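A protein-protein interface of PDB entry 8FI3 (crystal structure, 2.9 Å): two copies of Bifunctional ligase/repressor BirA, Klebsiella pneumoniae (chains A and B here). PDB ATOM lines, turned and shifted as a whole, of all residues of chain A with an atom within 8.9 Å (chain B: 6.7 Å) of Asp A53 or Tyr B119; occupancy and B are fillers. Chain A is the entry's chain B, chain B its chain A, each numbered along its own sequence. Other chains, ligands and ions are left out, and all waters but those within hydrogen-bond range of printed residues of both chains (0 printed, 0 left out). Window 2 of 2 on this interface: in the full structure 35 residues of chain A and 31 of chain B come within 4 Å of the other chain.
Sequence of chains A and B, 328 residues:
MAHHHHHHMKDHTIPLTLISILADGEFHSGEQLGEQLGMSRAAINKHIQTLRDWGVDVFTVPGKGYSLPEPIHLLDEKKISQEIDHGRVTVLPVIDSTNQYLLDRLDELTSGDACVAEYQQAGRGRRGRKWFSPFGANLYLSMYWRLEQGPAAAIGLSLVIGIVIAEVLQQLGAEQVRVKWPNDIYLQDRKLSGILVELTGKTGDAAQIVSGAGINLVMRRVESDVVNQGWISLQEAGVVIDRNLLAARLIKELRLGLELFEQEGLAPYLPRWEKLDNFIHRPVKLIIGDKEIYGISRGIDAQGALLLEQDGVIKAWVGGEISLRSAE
O of Trp A54 sits at hydrogen-bond distance from N of Phe B135, at 2.9 Å.
The side-chain carboxylate of Glu B118 is in hydrogen-bond range of the backbone NH of Leu A75 (2.8 Å).
N of Ala B117 sits at hydrogen-bond distance from O of Tyr B140, at 3.1 Å.
OE1 of Glu B118 lies within salt-bridge range of NH2 of Arg B243, 2.5 Å away.
OH of Tyr B140 lies within hydrogen-bond range of O of Pro B134, 2.9 Å away.
The backbone NH (N) of Ile B95 lies within hydrogen-bond range of the backbone carbonyl oxygen (O) of Tyr B119 (3.3 Å).
The backbone carbonyl oxygen (O) of Glu B118 lies within hydrogen-bond range of the backbone NH (N) of Gly B136 (2.9 Å).
O of Leu B92 is in hydrogen-bond range of N of Glu B118 (3.2 Å).
Val B94 touches His A12.
CB of Pro B93 touches CD2 of Leu A16, 3.5 Å away.
Leu A16 touches Phe B135 (CD2 to CE2, 3.7 Å).
Tyr B119 touches Asp A53.
Tyr B119 touches Trp A54 (CE1 to O, 3.4 Å).
Trp A54 touches Pro B134 (O to CA, 3.3 Å).
Pro B134 touches Gly A55.
CB of Phe B135 touches CG2 of Val A56 (3.6 Å).
Leu A75 touches Ala B117.
NH2 of Arg B243 touches CG of Leu A75 (3.5 Å).
Of the printed residues of chain B, His A12 touches Val B94.
Asn A45 touches none of the printed residues of chain B.
Of chain B, only Tyr B119 (3.97 Å) comes within 4 Å of Asp A53.
Printed residues of chain B within 4 Å of Gly A55: Pro B134 (3.5 Å).
Of the printed residues of chain B, Val A56 touches Phe B135.
Tyr B119 touches just these residues of chain A: Asp A53 (3.97 Å) and Trp A54 (3.4 Å).
Ala B122 touches none of the printed residues of chain A.
Printed residues of chain A within 4 Å of Arg B243: Leu A75 (3.5 Å).
The nearest residue of chain A that does not touch Tyr B119 is Gly A55 (5.1 Å).
The nearest printed residue of chain A that does not touch Pro B134 is Val A56 (5.1 Å).
Of the 19 printed residues of chain B, 8 touch a printed residue of chain A.
Printed residues of chain A that touch a printed residue of chain B: His A12, Leu A16, Asp A53, Trp A54, Gly A55, Val A56 and Leu A75.
Along chain A the printed residues that touch a printed residue of chain B span positions 12 to 75.
Among the printed residues, 13 pairs touch across the chains.
No position is printed for both chains.
Of the 13 pairs that touch across the chains among the printed residues, none has its exchanged pair printed and touching as well.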
ATOM      1  N   HIS A  12     -10.174  23.842  36.973  1.00  0.00           N
ATOM      2  CA  HIS A  12      -9.663  22.595  36.418  1.00  0.00           C
ATOM      3  C   HIS A  12      -8.142  22.545  36.506  1.00  0.00           C
ATOM      4  O   HIS A  12      -7.487  21.928  35.666  1.00  0.00           O
ATOM      5  CB  HIS A  12     -10.131  22.409  34.974  1.00  0.00           C
ATOM      6  CG  HIS A  12     -11.618  22.337  34.824  1.00  0.00           C
ATOM      7  ND1 HIS A  12     -12.399  21.455  35.539  1.00  0.00           N
ATOM      8  CD2 HIS A  12     -12.469  23.039  34.037  1.00  0.00           C
ATOM      9  CE1 HIS A  12     -13.666  21.617  35.201  1.00  0.00           C
ATOM     10  NE2 HIS A  12     -13.736  22.573  34.291  1.00  0.00           N
ATOM     11  N   LEU A  16      -5.559  20.213  34.231  1.00  0.00           N
ATOM     12  CA  LEU A  16      -4.836  20.976  33.218  1.00  0.00           C
ATOM     13  C   LEU A  16      -3.331  20.882  33.422  1.00  0.00           C
ATOM     14  O   LEU A  16      -2.573  20.783  32.451  1.00  0.00           O
ATOM     15  CB  LEU A  16      -5.289  22.433  33.232  1.00  0.00           C
ATOM     16  CG  LEU A  16      -6.692  22.673  32.676  1.00  0.00           C
ATOM     17  CD1 LEU A  16      -7.203  24.050  33.071  1.00  0.00           C
ATOM     18  CD2 LEU A  16      -6.696  22.492  31.169  1.00  0.00           C
ATOM     19  N   ASN A  45      -4.723   9.060  39.970  1.00  0.00           N
ATOM     20  CA  ASN A  45      -5.503   8.242  39.050  1.00  0.00           C
ATOM     21  C   ASN A  45      -6.861   8.875  38.773  1.00  0.00           C
ATOM     22  O   ASN A  45      -7.353   8.836  37.640  1.00  0.00           O
ATOM     23  CB  ASN A  45      -5.672   6.836  39.622  1.00  0.00           C
ATOM     24  CG  ASN A  45      -6.040   5.818  38.566  1.00  0.00           C
ATOM     25  OD1 ASN A  45      -5.171   5.188  37.966  1.00  0.00           O
ATOM     26  ND2 ASN A  45      -7.338   5.655  38.328  1.00  0.00           N
ATOM     27  N   LYS A  46      -7.484   9.456  39.803  1.00  0.00           N
ATOM     28  CA  LYS A  46      -8.792  10.078  39.629  1.00  0.00           C
ATOM     29  C   LYS A  46      -8.725  11.270  38.682  1.00  0.00           C
ATOM     30  O   LYS A  46      -9.654  11.502  37.901  1.00  0.00           O
ATOM     31  CB  LYS A  46      -9.361  10.500  40.982  1.00  0.00           C
ATOM     32  CG  LYS A  46     -10.450   9.575  41.499  1.00  0.00           C
ATOM     33  CD  LYS A  46     -11.469  10.332  42.334  1.00  0.00           C
ATOM     34  CE  LYS A  46     -12.720  10.642  41.526  1.00  0.00           C
ATOM     35  NZ  LYS A  46     -13.592  11.638  42.207  1.00  0.00           N
ATOM     36  N   HIS A  47      -7.654  12.059  38.753  1.00  0.00           N
ATOM     37  CA  HIS A  47      -7.549  13.194  37.843  1.00  0.00           C
ATOM     38  C   HIS A  47      -7.110  12.764  36.450  1.00  0.00           C
ATOM     39  O   HIS A  47      -7.398  13.463  35.472  1.00  0.00           O
ATOM     40  CB  HIS A  47      -6.607  14.244  38.427  1.00  0.00           C
ATOM     41  CG  HIS A  47      -7.260  15.127  39.441  1.00  0.00           C
ATOM     42  ND1 HIS A  47      -6.614  15.569  40.575  1.00  0.00           N
ATOM     43  CD2 HIS A  47      -8.511  15.646  39.493  1.00  0.00           C
ATOM     44  CE1 HIS A  47      -7.437  16.324  41.282  1.00  0.00           C
ATOM     45  NE2 HIS A  47      -8.592  16.386  40.646  1.00  0.00           N
ATOM     46  N   ILE A  48      -6.414  11.630  36.339  1.00  0.00           N
ATOM     47  CA  ILE A  48      -6.277  10.977  35.041  1.00  0.00           C
ATOM     48  C   ILE A  48      -7.650  10.553  34.537  1.00  0.00           C
ATOM     49  O   ILE A  48      -7.931  10.611  33.334  1.00  0.00           O
ATOM     50  CB  ILE A  48      -5.296   9.788  35.136  1.00  0.00           C
ATOM     51  CG1 ILE A  48      -3.864  10.251  34.866  1.00  0.00           C
ATOM     52  CG2 ILE A  48      -5.677   8.680  34.166  1.00  0.00           C
ATOM     53  CD1 ILE A  48      -3.618  10.697  33.438  1.00  0.00           C
ATOM     54  N   GLN A  49      -8.534  10.146  35.453  1.00  0.00           N
ATOM     55  CA  GLN A  49      -9.856   9.669  35.063  1.00  0.00           C
ATOM     56  C   GLN A  49     -10.703  10.796  34.487  1.00  0.00           C
ATOM     57  O   GLN A  49     -11.478  10.579  33.548  1.00  0.00           O
ATOM     58  CB  GLN A  49     -10.559   9.046  36.270  1.00  0.00           C
ATOM     59  N   THR A  50     -10.582  12.005  35.044  1.00  0.00           N
ATOM     60  CA  THR A  50     -11.284  13.156  34.479  1.00  0.00           C
ATOM     61  C   THR A  50     -10.817  13.450  33.059  1.00  0.00           C
ATOM     62  O   THR A  50     -11.628  13.791  32.191  1.00  0.00           O
ATOM     63  CB  THR A  50     -11.094  14.387  35.366  1.00  0.00           C
ATOM     64  OG1 THR A  50      -9.747  14.434  35.848  1.00  0.00           O
ATOM     65  CG2 THR A  50     -12.049  14.344  36.548  1.00  0.00           C
ATOM     66  N   LEU A  51      -9.510  13.328  32.805  1.00  0.00           N
ATOM     67  CA  LEU A  51      -8.977  13.637  31.480  1.00  0.00           C
ATOM     68  C   LEU A  51      -9.544  12.709  30.413  1.00  0.00           C
ATOM     69  O   LEU A  51      -9.833  13.146  29.293  1.00  0.00           O
ATOM     70  CB  LEU A  51      -7.452  13.563  31.502  1.00  0.00           C
ATOM     71  CG  LEU A  51      -6.719  14.779  32.072  1.00  0.00           C
ATOM     72  CD1 LEU A  51      -5.221  14.660  31.843  1.00  0.00           C
ATOM     73  CD2 LEU A  51      -7.257  16.068  31.470  1.00  0.00           C
ATOM     74  N   ARG A  52      -9.706  11.423  30.734  1.00  0.00           N
ATOM     75  CA  ARG A  52     -10.280  10.504  29.760  1.00  0.00           C
ATOM     76  C   ARG A  52     -11.752  10.807  29.515  1.00  0.00           C
ATOM     77  O   ARG A  52     -12.258  10.568  28.412  1.00  0.00           O
ATOM     78  CB  ARG A  52     -10.097   9.059  30.219  1.00  0.00           C
ATOM     79  CG  ARG A  52      -9.125   8.275  29.358  1.00  0.00           C
ATOM     80  CD  ARG A  52      -9.199   6.788  29.645  1.00  0.00           C
ATOM     81  NE  ARG A  52      -8.299   6.406  30.726  1.00  0.00           N
ATOM     82  CZ  ARG A  52      -7.701   5.226  30.819  1.00  0.00           C
ATOM     83  NH1 ARG A  52      -7.878   4.286  29.905  1.00  0.00           N
ATOM     84  NH2 ARG A  52      -6.902   4.984  31.856  1.00  0.00           N
ATOM     85  N   ASP A  53     -12.454  11.334  30.522  1.00  0.00           N
ATOM     86  CA  ASP A  53     -13.814  11.817  30.327  1.00  0.00           C
ATOM     87  C   ASP A  53     -13.867  13.052  29.440  1.00  0.00           C
ATOM     88  O   ASP A  53     -14.955  13.419  28.978  1.00  0.00           O
ATOM     89  CB  ASP A  53     -14.466  12.118  31.676  1.00  0.00           C
ATOM     90  CG  ASP A  53     -14.530  10.899  32.572  1.00  0.00           C
ATOM     91  OD1 ASP A  53     -14.606   9.772  32.038  1.00  0.00           O
ATOM     92  OD2 ASP A  53     -14.498  11.066  33.809  1.00  0.00           O
ATOM     93  N   TRP A  54     -12.729  13.701  29.198  1.00  0.00           N
ATOM     94  CA  TRP A  54     -12.641  14.834  28.290  1.00  0.00           C
ATOM     95  C   TRP A  54     -12.267  14.415  26.874  1.00  0.00           C
ATOM     96  O   TRP A  54     -12.037  15.279  26.023  1.00  0.00           O
ATOM     97  CB  TRP A  54     -11.619  15.851  28.809  1.00  0.00           C
ATOM     98  CG  TRP A  54     -12.064  16.607  30.025  1.00  0.00           C
ATOM     99  CD1 TRP A  54     -13.231  16.447  30.711  1.00  0.00           C
ATOM    100  CD2 TRP A  54     -11.342  17.646  30.698  1.00  0.00           C
ATOM    101  NE1 TRP A  54     -13.281  17.321  31.771  1.00  0.00           N
ATOM    102  CE2 TRP A  54     -12.133  18.068  31.784  1.00  0.00           C
ATOM    103  CE3 TRP A  54     -10.104  18.261  30.488  1.00  0.00           C
ATOM    104  CZ2 TRP A  54     -11.728  19.076  32.656  1.00  0.00           C
ATOM    105  CZ3 TRP A  54      -9.702  19.261  31.355  1.00  0.00           C
ATOM    106  CH2 TRP A  54     -10.511  19.658  32.425  1.00  0.00           C
ATOM    107  N   GLY A  55     -12.199  13.113  26.608  1.00  0.00           N
ATOM    108  CA  GLY A  55     -11.871  12.623  25.285  1.00  0.00           C
ATOM    109  C   GLY A  55     -10.397  12.470  24.996  1.00  0.00           C
ATOM    110  O   GLY A  55     -10.019  12.378  23.823  1.00  0.00           O
ATOM    111  N   VAL A  56      -9.550  12.438  26.019  1.00  0.00           N
ATOM    112  CA  VAL A  56      -8.112  12.294  25.829  1.00  0.00           C
ATOM    113  C   VAL A  56      -7.754  10.819  25.945  1.00  0.00           C
ATOM    114  O   VAL A  56      -8.064  10.172  26.950  1.00  0.00           O
ATOM    115  CB  VAL A  56      -7.328  13.134  26.849  1.00  0.00           C
ATOM    116  CG1 VAL A  56      -5.885  12.664  26.929  1.00  0.00           C
ATOM    117  CG2 VAL A  56      -7.390  14.603  26.480  1.00  0.00           C
ATOM    118  N   ASP A  57      -7.101  10.287  24.914  1.00  0.00           N
ATOM    119  CA  ASP A  57      -6.634   8.908  24.950  1.00  0.00           C
ATOM    120  C   ASP A  57      -5.422   8.807  25.866  1.00  0.00           C
ATOM    121  O   ASP A  57      -4.385   9.427  25.606  1.00  0.00           O
ATOM    122  CB  ASP A  57      -6.291   8.428  23.541  1.00  0.00           C
ATOM    123  CG  ASP A  57      -6.697   6.986  23.302  1.00  0.00           C
ATOM    124  OD1 ASP A  57      -6.160   6.092  23.988  1.00  0.00           O
ATOM    125  OD2 ASP A  57      -7.557   6.747  22.426  1.00  0.00           O
ATOM    126  N   VAL A  58      -5.551   8.031  26.938  1.00  0.00           N
ATOM    127  CA  VAL A  58      -4.495   7.857  27.925  1.00  0.00           C
ATOM    128  C   VAL A  58      -4.237   6.370  28.087  1.00  0.00           C
ATOM    129  O   VAL A  58      -5.178   5.590  28.276  1.00  0.00           O
ATOM    130  CB  VAL A  58      -4.866   8.485  29.283  1.00  0.00           C
ATOM    131  CG1 VAL A  58      -3.768   8.227  30.306  1.00  0.00           C
ATOM    132  CG2 VAL A  58      -5.114   9.973  29.134  1.00  0.00           C
ATOM    133  N   LEU A  75      -2.468  24.512  22.810  1.00  0.00           N
ATOM    134  CA  LEU A  75      -2.665  25.870  22.333  1.00  0.00           C
ATOM    135  C   LEU A  75      -1.992  26.866  23.271  1.00  0.00           C
ATOM    136  O   LEU A  75      -2.089  26.755  24.496  1.00  0.00           O
ATOM    137  CB  LEU A  75      -4.158  26.183  22.220  1.00  0.00           C
ATOM    138  CG  LEU A  75      -4.974  25.325  21.251  1.00  0.00           C
ATOM    139  CD1 LEU A  75      -6.463  25.575  21.441  1.00  0.00           C
ATOM    140  CD2 LEU A  75      -4.563  25.595  19.813  1.00  0.00           C
ATOM    141  N   LEU B  92      -8.862  29.376  25.476  1.00  0.00           N
ATOM    142  CA  LEU B  92      -9.539  28.887  26.667  1.00  0.00           C
ATOM    143  C   LEU B  92      -9.298  27.391  26.795  1.00  0.00           C
ATOM    144  O   LEU B  92      -9.640  26.634  25.868  1.00  0.00           O
ATOM    145  CB  LEU B  92     -11.035  29.191  26.605  1.00  0.00           C
ATOM    146  CG  LEU B  92     -11.410  30.594  27.079  1.00  0.00           C
ATOM    147  CD1 LEU B  92     -12.731  31.014  26.474  1.00  0.00           C
ATOM    148  CD2 LEU B  92     -11.463  30.656  28.600  1.00  0.00           C
ATOM    149  N   PRO B  93      -8.706  26.916  27.892  1.00  0.00           N
ATOM    150  CA  PRO B  93      -8.532  25.460  28.042  1.00  0.00           C
ATOM    151  C   PRO B  93      -9.853  24.711  28.096  1.00  0.00           C
ATOM    152  O   PRO B  93     -10.038  23.727  27.367  1.00  0.00           O
ATOM    153  CB  PRO B  93      -7.743  25.340  29.354  1.00  0.00           C
ATOM    154  CG  PRO B  93      -7.132  26.689  29.573  1.00  0.00           C
ATOM    155  CD  PRO B  93      -8.109  27.667  29.007  1.00  0.00           C
ATOM    156  N   VAL B  94     -10.782  25.148  28.942  1.00  0.00           N
ATOM    157  CA  VAL B  94     -12.087  24.515  29.079  1.00  0.00           C
ATOM    158  C   VAL B  94     -13.157  25.590  28.973  1.00  0.00           C
ATOM    159  O   VAL B  94     -13.071  26.625  29.642  1.00  0.00           O
ATOM    160  CB  VAL B  94     -12.219  23.749  30.411  1.00  0.00           C
ATOM    161  CG1 VAL B  94     -13.620  23.178  30.563  1.00  0.00           C
ATOM    162  CG2 VAL B  94     -11.178  22.644  30.495  1.00  0.00           C
ATOM    163  N   ILE B  95     -14.161  25.342  28.133  1.00  0.00           N
ATOM    164  CA  ILE B  95     -15.285  26.256  27.967  1.00  0.00           C
ATOM    165  C   ILE B  95     -16.460  25.439  27.456  1.00  0.00           C
ATOM    166  O   ILE B  95     -16.284  24.351  26.907  1.00  0.00           O
ATOM    167  CB  ILE B  95     -14.936  27.424  27.007  1.00  0.00           C
ATOM    168  CG1 ILE B  95     -15.830  28.632  27.287  1.00  0.00           C
ATOM    169  CG2 ILE B  95     -15.059  26.984  25.556  1.00  0.00           C
ATOM    170  CD1 ILE B  95     -15.777  29.114  28.719  1.00  0.00           C
ATOM    171  N   ASP B  96     -17.674  25.957  27.655  1.00  0.00           N
ATOM    172  CA  ASP B  96     -18.850  25.275  27.123  1.00  0.00           C
ATOM    173  C   ASP B  96     -18.875  25.330  25.599  1.00  0.00           C
ATOM    174  O   ASP B  96     -19.081  24.309  24.933  1.00  0.00           O
ATOM    175  CB  ASP B  96     -20.124  25.886  27.710  1.00  0.00           C
ATOM    176  CG  ASP B  96     -20.150  27.399  27.607  1.00  0.00           C
ATOM    177  OD1 ASP B  96     -19.064  28.010  27.498  1.00  0.00           O
ATOM    178  OD2 ASP B  96     -21.256  27.978  27.639  1.00  0.00           O
ATOM    179  N   SER B  97     -18.657  26.513  25.030  1.00  0.00           N
ATOM    180  CA  SER B  97     -18.593  26.677  23.583  1.00  0.00           C
ATOM    181  C   SER B  97     -17.861  27.971  23.265  1.00  0.00           C
ATOM    182  O   SER B  97     -18.024  28.970  23.971  1.00  0.00           O
ATOM    183  CB  SER B  97     -19.993  26.695  22.962  1.00  0.00           C
ATOM    184  OG  SER B  97     -19.920  26.598  21.550  1.00  0.00           O
ATOM    185  N   ALA B 117     -10.450  27.132  21.719  1.00  0.00           N
ATOM    186  CA  ALA B 117     -10.570  26.280  22.890  1.00  0.00           C
ATOM    187  C   ALA B 117      -9.949  24.920  22.611  1.00  0.00           C
ATOM    188  O   ALA B 117      -9.951  24.436  21.476  1.00  0.00           O
ATOM    189  CB  ALA B 117     -12.032  26.103  23.316  1.00  0.00           C
ATOM    190  N   GLU B 118      -9.408  24.309  23.665  1.00  0.00           N
ATOM    191  CA  GLU B 118      -8.889  22.950  23.583  1.00  0.00           C
ATOM    192  C   GLU B 118      -9.982  21.917  23.811  1.00  0.00           C
ATOM    193  O   GLU B 118      -9.968  20.849  23.188  1.00  0.00           O
ATOM    194  CB  GLU B 118      -7.764  22.750  24.602  1.00  0.00           C
ATOM    195  CG  GLU B 118      -6.604  23.719  24.447  1.00  0.00           C
ATOM    196  CD  GLU B 118      -5.280  23.011  24.225  1.00  0.00           C
ATOM    197  OE1 GLU B 118      -5.273  21.957  23.553  1.00  0.00           O
ATOM    198  OE2 GLU B 118      -4.246  23.507  24.720  1.00  0.00           O
ATOM    199  N   TYR B 119     -10.935  22.223  24.688  1.00  0.00           N
ATOM    200  CA  TYR B 119     -12.014  21.311  25.039  1.00  0.00           C
ATOM    201  C   TYR B 119     -13.292  22.114  25.185  1.00  0.00           C
ATOM    202  O   TYR B 119     -13.322  23.102  25.923  1.00  0.00           O
ATOM    203  CB  TYR B 119     -11.691  20.570  26.343  1.00  0.00           C
ATOM    204  CG  TYR B 119     -12.792  19.692  26.897  1.00  0.00           C
ATOM    205  CD1 TYR B 119     -13.231  18.571  26.208  1.00  0.00           C
ATOM    206  CD2 TYR B 119     -13.374  19.972  28.128  1.00  0.00           C
ATOM    207  CE1 TYR B 119     -14.230  17.762  26.720  1.00  0.00           C
ATOM    208  CE2 TYR B 119     -14.372  19.167  28.648  1.00  0.00           C
ATOM    209  CZ  TYR B 119     -14.797  18.064  27.938  1.00  0.00           C
ATOM    210  OH  TYR B 119     -15.790  17.262  28.451  1.00  0.00           O
ATOM    211  N   GLN B 120     -14.341  21.695  24.483  1.00  0.00           N
ATOM    212  CA  GLN B 120     -15.648  22.332  24.577  1.00  0.00           C
ATOM    213  C   GLN B 120     -16.597  21.377  25.286  1.00  0.00           C
ATOM    214  O   GLN B 120     -16.818  20.256  24.817  1.00  0.00           O
ATOM    215  CB  GLN B 120     -16.179  22.720  23.199  1.00  0.00           C
ATOM    216  CG  GLN B 120     -15.699  24.085  22.735  1.00  0.00           C
ATOM    217  CD  GLN B 120     -16.285  24.492  21.401  1.00  0.00           C
ATOM    218  OE1 GLN B 120     -16.375  25.679  21.089  1.00  0.00           O
ATOM    219  NE2 GLN B 120     -16.685  23.508  20.605  1.00  0.00           N
ATOM    220  N   GLN B 121     -17.153  21.805  26.413  1.00  0.00           N
ATOM    221  CA  GLN B 121     -18.024  20.910  27.215  1.00  0.00           C
ATOM    222  C   GLN B 121     -19.389  20.766  26.544  1.00  0.00           C
ATOM    223  O   GLN B 121     -19.981  19.686  26.666  1.00  0.00           O
ATOM    224  CB  GLN B 121     -18.179  21.473  28.625  1.00  0.00           C
ATOM    225  CG  GLN B 121     -16.872  21.942  29.241  1.00  0.00           C
ATOM    226  CD  GLN B 121     -16.977  22.050  30.741  1.00  0.00           C
ATOM    227  OE1 GLN B 121     -17.407  23.065  31.281  1.00  0.00           O
ATOM    228  NE2 GLN B 121     -16.580  20.993  31.428  1.00  0.00           N
ATOM    229  N   ALA B 122     -19.860  21.813  25.866  1.00  0.00           N
ATOM    230  CA  ALA B 122     -21.185  21.772  25.214  1.00  0.00           C
ATOM    231  C   ALA B 122     -21.075  22.259  23.770  1.00  0.00           C
ATOM    232  O   ALA B 122     -21.668  23.296  23.460  1.00  0.00           O
ATOM    233  CB  ALA B 122     -22.142  22.633  25.981  1.00  0.00           C
ATOM    234  N   SER B 133     -16.218  17.668  21.173  1.00  0.00           N
ATOM    235  CA  SER B 133     -14.957  18.405  21.124  1.00  0.00           C
ATOM    236  C   SER B 133     -14.032  17.864  22.202  1.00  0.00           C
ATOM    237  O   SER B 133     -13.908  18.453  23.284  1.00  0.00           O
ATOM    238  CB  SER B 133     -15.194  19.905  21.302  1.00  0.00           C
ATOM    239  OG  SER B 133     -16.241  20.365  20.469  1.00  0.00           O
ATOM    240  N   PRO B 134     -13.368  16.741  21.943  1.00  0.00           N
ATOM    241  CA  PRO B 134     -12.403  16.213  22.912  1.00  0.00           C
ATOM    242  C   PRO B 134     -11.213  17.143  23.087  1.00  0.00           C
ATOM    243  O   PRO B 134     -10.853  17.911  22.193  1.00  0.00           O
ATOM    244  CB  PRO B 134     -11.980  14.871  22.299  1.00  0.00           C
ATOM    245  CG  PRO B 134     -12.281  15.006  20.843  1.00  0.00           C
ATOM    246  CD  PRO B 134     -13.499  15.871  20.760  1.00  0.00           C
ATOM    247  N   PHE B 135     -10.605  17.064  24.272  1.00  0.00           N
ATOM    248  CA  PHE B 135      -9.519  17.967  24.635  1.00  0.00           C
ATOM    249  C   PHE B 135      -8.314  17.785  23.718  1.00  0.00           C
ATOM    250  O   PHE B 135      -7.858  16.662  23.484  1.00  0.00           O
ATOM    251  CB  PHE B 135      -9.111  17.732  26.092  1.00  0.00           C
ATOM    252  CG  PHE B 135      -8.207  18.801  26.659  1.00  0.00           C
ATOM    253  CD1 PHE B 135      -6.875  18.883  26.283  1.00  0.00           C
ATOM    254  CD2 PHE B 135      -8.692  19.716  27.579  1.00  0.00           C
ATOM    255  CE1 PHE B 135      -6.051  19.862  26.803  1.00  0.00           C
ATOM    256  CE2 PHE B 135      -7.872  20.697  28.104  1.00  0.00           C
ATOM    257  CZ  PHE B 135      -6.551  20.769  27.715  1.00  0.00           C
ATOM    258  N   GLY B 136      -7.800  18.904  23.211  1.00  0.00           N
ATOM    259  CA  GLY B 136      -6.524  18.924  22.512  1.00  0.00           C
ATOM    260  C   GLY B 136      -6.453  18.045  21.285  1.00  0.00           C
ATOM    261  O   GLY B 136      -5.365  17.577  20.931  1.00  0.00           O
ATOM    262  N   ASN B 138      -8.933  18.513  18.105  1.00  0.00           N
ATOM    263  CA  ASN B 138      -9.314  19.262  16.919  1.00  0.00           C
ATOM    264  C   ASN B 138      -9.308  20.754  17.231  1.00  0.00           C
ATOM    265  O   ASN B 138      -9.076  21.174  18.367  1.00  0.00           O
ATOM    266  CB  ASN B 138     -10.687  18.807  16.421  1.00  0.00           C
ATOM    267  CG  ASN B 138     -10.706  17.345  16.025  1.00  0.00           C
ATOM    268  OD1 ASN B 138      -9.964  16.919  15.141  1.00  0.00           O
ATOM    269  ND2 ASN B 138     -11.554  16.565  16.685  1.00  0.00           N
ATOM    270  N   TYR B 140     -11.240  24.244  17.632  1.00  0.00           N
ATOM    271  CA  TYR B 140     -12.540  24.806  17.984  1.00  0.00           C
ATOM    272  C   TYR B 140     -12.358  26.320  18.040  1.00  0.00           C
ATOM    273  O   TYR B 140     -11.947  26.877  19.061  1.00  0.00           O
ATOM    274  CB  TYR B 140     -13.040  24.223  19.300  1.00  0.00           C
ATOM    275  CG  TYR B 140     -12.782  22.738  19.404  1.00  0.00           C
ATOM    276  CD1 TYR B 140     -13.326  21.857  18.476  1.00  0.00           C
ATOM    277  CD2 TYR B 140     -11.978  22.217  20.411  1.00  0.00           C
ATOM    278  CE1 TYR B 140     -13.087  20.499  18.556  1.00  0.00           C
ATOM    279  CE2 TYR B 140     -11.734  20.858  20.498  1.00  0.00           C
ATOM    280  CZ  TYR B 140     -12.289  20.004  19.566  1.00  0.00           C
ATOM    281  OH  TYR B 140     -12.053  18.651  19.647  1.00  0.00           O
ATOM    282  N   ARG B 243      -1.676  22.889  15.630  1.00  0.00           N
ATOM    283  CA  ARG B 243      -2.947  23.544  15.922  1.00  0.00           C
ATOM    284  C   ARG B 243      -2.762  25.039  16.149  1.00  0.00           C
ATOM    285  O   ARG B 243      -3.604  25.845  15.734  1.00  0.00           O
ATOM    286  CB  ARG B 243      -3.616  22.887  17.131  1.00  0.00           C
ATOM    287  CG  ARG B 243      -4.640  21.832  16.748  1.00  0.00           C
ATOM    288  CD  ARG B 243      -4.727  20.721  17.780  1.00  0.00           C
ATOM    289  NE  ARG B 243      -5.476  21.130  18.960  1.00  0.00           N
ATOM    290  CZ  ARG B 243      -4.923  21.514  20.102  1.00  0.00           C
ATOM    291  NH1 ARG B 243      -3.609  21.553  20.255  1.00  0.00           N
ATOM    292  NH2 ARG B 243      -5.708  21.869  21.116  1.00  0.00           N
